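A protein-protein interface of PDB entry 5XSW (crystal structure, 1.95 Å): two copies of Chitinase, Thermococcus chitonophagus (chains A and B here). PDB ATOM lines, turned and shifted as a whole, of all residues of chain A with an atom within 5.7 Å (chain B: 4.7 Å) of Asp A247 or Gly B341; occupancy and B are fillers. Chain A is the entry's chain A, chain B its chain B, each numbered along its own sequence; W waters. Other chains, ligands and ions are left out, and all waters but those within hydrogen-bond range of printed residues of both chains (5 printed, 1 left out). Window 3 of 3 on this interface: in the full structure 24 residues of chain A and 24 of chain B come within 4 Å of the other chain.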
ATOM      1  N   HIS A 245      21.933   8.102 -24.211  1.00  0.00           N
ATOM      2  CA  HIS A 245      22.282   6.708 -23.857  1.00  0.00           C
ATOM      3  C   HIS A 245      23.655   6.652 -23.189  1.00  0.00           C
ATOM      4  O   HIS A 245      24.619   7.209 -23.695  1.00  0.00           O
ATOM      5  CB  HIS A 245      22.250   5.840 -25.108  1.00  0.00           C
ATOM      6  CG  HIS A 245      22.119   4.383 -24.807  1.00  0.00           C
ATOM      7  ND1 HIS A 245      23.100   3.691 -24.132  1.00  0.00           N
ATOM      8  CD2 HIS A 245      21.109   3.499 -25.036  1.00  0.00           C
ATOM      9  CE1 HIS A 245      22.735   2.416 -24.015  1.00  0.00           C
ATOM     10  NE2 HIS A 245      21.526   2.278 -24.539  1.00  0.00           N
ATOM     11  N   PRO A 246      23.758   6.012 -22.017  1.00  0.00           N
ATOM     12  CA  PRO A 246      25.041   5.972 -21.300  1.00  0.00           C
ATOM     13  C   PRO A 246      26.141   5.298 -22.126  1.00  0.00           C
ATOM     14  O   PRO A 246      27.309   5.558 -21.869  1.00  0.00           O
ATOM     15  CB  PRO A 246      24.752   5.082 -20.054  1.00  0.00           C
ATOM     16  CG  PRO A 246      23.167   5.242 -19.883  1.00  0.00           C
ATOM     17  CD  PRO A 246      22.674   5.311 -21.305  1.00  0.00           C
ATOM     18  N   ASP A 247      25.766   4.464 -23.083  1.00  0.00           N
ATOM     19  CA  ASP A 247      26.840   3.793 -23.883  1.00  0.00           C
ATOM     20  C   ASP A 247      27.219   4.626 -25.134  1.00  0.00           C
ATOM     21  O   ASP A 247      28.073   4.192 -25.894  1.00  0.00           O
ATOM     22  CB  ASP A 247      26.404   2.373 -24.303  1.00  0.00           C
ATOM     23  CG  ASP A 247      26.132   1.468 -23.069  1.00  0.00           C
ATOM     24  OD1 ASP A 247      26.642   1.755 -21.992  1.00  0.00           O
ATOM     25  OD2 ASP A 247      25.425   0.485 -23.215  1.00  0.00           O
ATOM     26  N   GLY A 248      26.584   5.784 -25.350  1.00  0.00           N
ATOM     27  CA  GLY A 248      27.092   6.720 -26.368  1.00  0.00           C
ATOM     28  C   GLY A 248      26.718   6.314 -27.769  1.00  0.00           C
ATOM     29  O   GLY A 248      25.948   5.376 -27.986  1.00  0.00           O
ATOM     30  N   ILE A 249      27.292   6.995 -28.756  1.00  0.00           N
ATOM     31  CA  ILE A 249      26.875   6.728 -30.127  1.00  0.00           C
ATOM     32  C   ILE A 249      27.549   5.468 -30.675  1.00  0.00           C
ATOM     33  O   ILE A 249      27.083   4.946 -31.649  1.00  0.00           O
ATOM     34  CB  ILE A 249      27.183   7.911 -31.049  1.00  0.00           C
ATOM     35  CG1 ILE A 249      28.680   8.280 -31.040  1.00  0.00           C
ATOM     36  CG2 ILE A 249      26.377   9.213 -30.592  1.00  0.00           C
ATOM     37  CD1 ILE A 249      29.037   9.380 -32.154  1.00  0.00           C
ATOM     38  N   PHE A 250      28.618   5.008 -30.046  1.00  0.00           N
ATOM     39  CA  PHE A 250      29.287   3.714 -30.428  1.00  0.00           C
ATOM     40  C   PHE A 250      28.784   2.505 -29.657  1.00  0.00           C
ATOM     41  O   PHE A 250      29.182   1.376 -29.948  1.00  0.00           O
ATOM     42  CB  PHE A 250      30.797   3.862 -30.168  1.00  0.00           C
ATOM     43  CG  PHE A 250      31.420   4.902 -31.085  1.00  0.00           C
ATOM     44  CD1 PHE A 250      31.597   4.594 -32.451  1.00  0.00           C
ATOM     45  CD2 PHE A 250      31.706   6.189 -30.598  1.00  0.00           C
ATOM     46  CE1 PHE A 250      32.161   5.554 -33.338  1.00  0.00           C
ATOM     47  CE2 PHE A 250      32.268   7.202 -31.468  1.00  0.00           C
ATOM     48  CZ  PHE A 250      32.511   6.860 -32.822  1.00  0.00           C
ATOM     49  N   GLN A 251      27.964   2.759 -28.619  1.00  0.00           N
ATOM     50  CA  GLN A 251      27.361   1.668 -27.777  1.00  0.00           C
ATOM     51  C   GLN A 251      28.423   0.803 -27.182  1.00  0.00           C
ATOM     52  O   GLN A 251      28.367  -0.426 -27.229  1.00  0.00           O
ATOM     53  CB  GLN A 251      26.349   0.834 -28.589  1.00  0.00           C
ATOM     54  CG  GLN A 251      25.158   1.748 -29.067  1.00  0.00           C
ATOM     55  CD  GLN A 251      24.142   1.974 -27.893  1.00  0.00           C
ATOM     56  OE1 GLN A 251      23.410   1.040 -27.546  1.00  0.00           O
ATOM     57  NE2 GLN A 251      24.161   3.158 -27.254  1.00  0.00           N
ATOM     58  N   VAL A 252      29.434   1.450 -26.635  1.00  0.00           N
ATOM     59  CA  VAL A 252      30.454   0.738 -25.883  1.00  0.00           C
ATOM     60  C   VAL A 252      29.884   0.494 -24.444  1.00  0.00           C
ATOM     61  O   VAL A 252      29.605   1.463 -23.748  1.00  0.00           O
ATOM     62  CB  VAL A 252      31.773   1.549 -25.757  1.00  0.00           C
ATOM     63  CG1 VAL A 252      32.759   0.786 -24.809  1.00  0.00           C
ATOM     64  CG2 VAL A 252      32.425   1.789 -27.177  1.00  0.00           C
ATOM     65  N   GLU A 253      29.791  -0.761 -24.015  1.00  0.00           N
ATOM     66  CA  GLU A 253      29.291  -1.092 -22.654  1.00  0.00           C
ATOM     67  C   GLU A 253      30.337  -1.018 -21.577  1.00  0.00           C
ATOM     68  O   GLU A 253      31.550  -1.057 -21.862  1.00  0.00           O
ATOM     69  CB  GLU A 253      28.675  -2.508 -22.680  1.00  0.00           C
ATOM     70  CG  GLU A 253      27.476  -2.522 -23.603  1.00  0.00           C
ATOM     71  CD  GLU A 253      26.714  -3.851 -23.580  1.00  0.00           C
ATOM     72  OE1 GLU A 253      26.681  -4.491 -22.509  1.00  0.00           O
ATOM     73  OE2 GLU A 253      26.172  -4.255 -24.629  1.00  0.00           O
ATOM     74  N   SER A 254      29.908  -0.956 -20.312  1.00  0.00           N
ATOM     75  CA  SER A 254      30.900  -0.817 -19.286  1.00  0.00           C
ATOM     76  C   SER A 254      31.841  -2.017 -19.125  1.00  0.00           C
ATOM     77  O   SER A 254      32.968  -1.797 -18.711  1.00  0.00           O
ATOM     78  CB  SER A 254      30.260  -0.465 -17.915  1.00  0.00           C
ATOM     79  OG  SER A 254      29.553  -1.548 -17.391  1.00  0.00           O
ATOM     80  N   HIS A 274      33.331   4.957 -17.413  1.00  0.00           N
ATOM     81  CA  HIS A 274      32.576   4.642 -18.634  1.00  0.00           C
ATOM     82  C   HIS A 274      31.603   5.745 -19.096  1.00  0.00           C
ATOM     83  O   HIS A 274      31.666   6.264 -20.258  1.00  0.00           O
ATOM     84  CB  HIS A 274      31.806   3.330 -18.427  1.00  0.00           C
ATOM     85  CG  HIS A 274      30.800   3.057 -19.507  1.00  0.00           C
ATOM     86  ND1 HIS A 274      29.486   3.492 -19.434  1.00  0.00           N
ATOM     87  CD2 HIS A 274      30.924   2.447 -20.702  1.00  0.00           C
ATOM     88  CE1 HIS A 274      28.852   3.157 -20.544  1.00  0.00           C
ATOM     89  NE2 HIS A 274      29.686   2.474 -21.308  1.00  0.00           N
ATOM     90  N   ASP A 275      30.656   6.117 -18.225  1.00  0.00           N
ATOM     91  CA  ASP A 275      29.644   7.101 -18.665  1.00  0.00           C
ATOM     92  C   ASP A 275      30.322   8.450 -18.958  1.00  0.00           C
ATOM     93  O   ASP A 275      29.986   9.124 -19.933  1.00  0.00           O
ATOM     94  CB  ASP A 275      28.469   7.260 -17.605  1.00  0.00           C
ATOM     95  CG  ASP A 275      27.555   5.982 -17.490  1.00  0.00           C
ATOM     96  OD1 ASP A 275      27.901   4.866 -17.972  1.00  0.00           O
ATOM     97  OD2 ASP A 275      26.478   6.057 -16.845  1.00  0.00           O
ATOM     98  N   MET A 278      31.880   8.019 -22.553  1.00  0.00           N
ATOM     99  CA  MET A 278      31.051   7.574 -23.672  1.00  0.00           C
ATOM    100  C   MET A 278      29.759   8.416 -23.835  1.00  0.00           C
ATOM    101  O   MET A 278      29.236   8.548 -24.939  1.00  0.00           O
ATOM    102  CB  MET A 278      30.620   6.113 -23.524  1.00  0.00           C
ATOM    103  CG  MET A 278      31.801   5.066 -23.353  1.00  0.00           C
ATOM    104  SD  MET A 278      33.038   5.377 -24.680  1.00  0.00           S
ATOM    105  CE  MET A 278      31.995   5.133 -26.003  1.00  0.00           C
ATOM    106  N   LYS A 279      29.219   8.925 -22.735  1.00  0.00           N
ATOM    107  CA  LYS A 279      27.873   9.506 -22.809  1.00  0.00           C
ATOM    108  C   LYS A 279      27.913  10.970 -23.325  1.00  0.00           C
ATOM    109  O   LYS A 279      28.400  11.867 -22.653  1.00  0.00           O
ATOM    110  CB  LYS A 279      27.175   9.455 -21.410  1.00  0.00           C
ATOM    111  CG  LYS A 279      25.673   9.980 -21.464  1.00  0.00           C
ATOM    112  CD  LYS A 279      25.136  10.035 -19.948  1.00  0.00           C
ATOM    113  CE  LYS A 279      23.656  10.487 -19.915  1.00  0.00           C
ATOM    114  NZ  LYS A 279      23.384  11.063 -18.561  1.00  0.00           N
ATOM    115  N   GLY B 339      22.995  -5.105 -21.025  1.00  0.00           N
ATOM    116  CA  GLY B 339      24.021  -4.400 -20.267  1.00  0.00           C
ATOM    117  C   GLY B 339      23.418  -3.430 -19.205  1.00  0.00           C
ATOM    118  O   GLY B 339      22.257  -3.077 -19.300  1.00  0.00           O
ATOM    119  N   VAL B 340      24.189  -3.011 -18.223  1.00  0.00           N
ATOM    120  CA  VAL B 340      23.626  -2.111 -17.181  1.00  0.00           C
ATOM    121  C   VAL B 340      23.441  -0.695 -17.709  1.00  0.00           C
ATOM    122  O   VAL B 340      22.704   0.083 -17.133  1.00  0.00           O
ATOM    123  CB  VAL B 340      24.515  -2.086 -15.889  1.00  0.00           C
ATOM    124  CG1 VAL B 340      24.556  -3.497 -15.205  1.00  0.00           C
ATOM    125  CG2 VAL B 340      25.975  -1.590 -16.174  1.00  0.00           C
ATOM    126  N   GLY B 341      24.117  -0.343 -18.812  1.00  0.00           N
ATOM    127  CA  GLY B 341      23.905   0.943 -19.464  1.00  0.00           C
ATOM    128  C   GLY B 341      22.505   0.993 -19.991  1.00  0.00           C
ATOM    129  O   GLY B 341      21.818   2.030 -19.883  1.00  0.00           O
ATOM    130  N   ALA B 342      22.070  -0.138 -20.559  1.00  0.00           N
ATOM    131  CA  ALA B 342      20.759  -0.206 -21.142  1.00  0.00           C
ATOM    132  C   ALA B 342      19.691  -0.106 -20.020  1.00  0.00           C
ATOM    133  O   ALA B 342      18.641   0.513 -20.227  1.00  0.00           O
ATOM    134  CB  ALA B 342      20.555  -1.516 -21.945  1.00  0.00           C
ATOM    135  N   ILE B 343      19.936  -0.744 -18.876  1.00  0.00           N
ATOM    136  CA  ILE B 343      18.991  -0.574 -17.721  1.00  0.00           C
ATOM    137  C   ILE B 343      18.947   0.920 -17.355  1.00  0.00           C
ATOM    138  O   ILE B 343      17.880   1.525 -17.201  1.00  0.00           O
ATOM    139  CB  ILE B 343      19.376  -1.370 -16.434  1.00  0.00           C
ATOM    140  CG1 ILE B 343      19.156  -2.892 -16.621  1.00  0.00           C
ATOM    141  CG2 ILE B 343      18.429  -0.932 -15.211  1.00  0.00           C
ATOM    142  CD1 ILE B 343      19.813  -3.745 -15.445  1.00  0.00           C
ATOM    143  N   GLU B 344      20.119   1.541 -17.270  1.00  0.00           N
ATOM    144  CA  GLU B 344      20.165   2.928 -16.794  1.00  0.00           C
ATOM    145  C   GLU B 344      19.371   3.859 -17.728  1.00  0.00           C
ATOM    146  O   GLU B 344      18.675   4.794 -17.283  1.00  0.00           O
ATOM    147  CB  GLU B 344      21.620   3.362 -16.649  1.00  0.00           C
ATOM    148  CG  GLU B 344      21.842   4.805 -16.231  1.00  0.00           C
ATOM    149  CD  GLU B 344      23.333   5.143 -16.152  1.00  0.00           C
ATOM    150  OE1 GLU B 344      24.202   4.468 -16.805  1.00  0.00           O
ATOM    151  OE2 GLU B 344      23.658   6.071 -15.408  1.00  0.00           O
ATOM    152  N   ALA B 345      19.416   3.591 -19.017  1.00  0.00           N
ATOM    153  CA  ALA B 345      18.763   4.455 -19.986  1.00  0.00           C
ATOM    154  C   ALA B 345      17.231   4.447 -19.808  1.00  0.00           C
ATOM    155  O   ALA B 345      16.549   5.403 -20.194  1.00  0.00           O
ATOM    156  CB  ALA B 345      19.124   4.010 -21.407  1.00  0.00           C
HETATM  157  O   HOH W   1      24.453  -1.509 -21.682  1.00  0.00           O
HETATM  158  O   HOH W   2      22.361   8.309 -17.415  1.00  0.00           O
HETATM  159  O   HOH W   3      27.250   0.535 -19.664  1.00  0.00           O
HETATM  160  O   HOH W   4      25.414  -6.955 -22.099  1.00  0.00           O
HETATM  161  O   HOH W   5      25.371   8.542 -15.947  1.00  0.00           O
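The side-chain carboxylate of Asp A275 lies close to the side-chain carboxylate of Glu B344.
OD1 of Asp A247 lies close to NE2 of His A274 (3.2 Å).
ND1 of His A274 is in hydrogen-bond range of OD1 of Asp A275.
ND1 of His A245 lies within hydrogen-bond range of N of Asp A247, at 3.0 Å.
The backbone NH of Val A252 sits at hydrogen-bond distance from the backbone carbonyl oxygen of Asp A247 (3.1 Å).
Printed residues of chain A that touch a printed residue of chain B: Pro A246, Asp A247, Glu A253, Ser A254 and Asp A275.
Hydrophobic or aromatic side chains of chain A within 4 Å of the printed part of chain B: Pro A246.
Printed residues of chain B that touch a printed residue of chain A: Gly B339, Val B340, Gly B341, Glu B344 and Ala B345.
Among the printed residues, 7 pairs touch across the chains.
No position is printed for both chains.
Of the 7 pairs that touch across the chains among the printed residues, none has its exchanged pair printed and touching as well.
Pro A246 touches Gly B341 (CG to O, 3.5 Å).
Pro A246 touches Glu B344 (CG to OE1, 3.3 Å).
Pro A246 touches Ala B345 (CD to CB, 3.8 Å).
Asp A247 touches Gly B341 (OD1 to CA, 3.8 Å).
Gly B339 touches Glu A253 (CA to OE1, 3.5 Å).
Val B340 touches Ser A254 (CG2 to OG, 3.8 Å).
Of chain B, only Gly B341 comes within 4 Å of Asp A247.
Of the printed residues of chain B, Glu A253 touches Gly B339.
Of the printed residues of chain B, Ser A254 touches Val B340.
Of the printed residues of chain B, Asp A275 touches Glu B344.
Met A278 touches none of the printed residues of chain B.
Lys A279 touches none of the printed residues of chain B.
Of chain A, only Pro A246 and Asp A247 come within 4 Å of Gly B341.
Of the printed residues of chain A, Glu B344 touches Pro A246 (3.3 Å) and Asp A275 (2.8 Å).
Printed residues of chain A within 4 Å of Ala B345: Pro A246.
The nearest residue of chain B that does not touch Asp A247 is Ala B342 (4.3 Å).
The nearest printed residue of chain A that does not touch Glu B344 is Lys A279 (5.9 Å).
Water W1 lies within hydrogen-bond range of the side-chain carboxylate (OD2) of Asp A247, the backbone NH (N) of Ala B342 and the backbone NH (N) of Gly B341.
Water W3 lies within hydrogen-bond range of OD1 of Asp A247, N of Ser A254 and N of Gly B341.
Water W4 lies within hydrogen-bond range of OE1 of Glu A253 and N of Gly B339.
Water W5 lies within hydrogen-bond range of OD2 of Asp A275 (2.9 Å) and OE2 of Glu B344 (3.1 Å).
Water W2 bridges the side-chain amino group of Lys A279 (3.2 Å) and the side-chain carboxylate of Glu B344 (3.3 Å).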
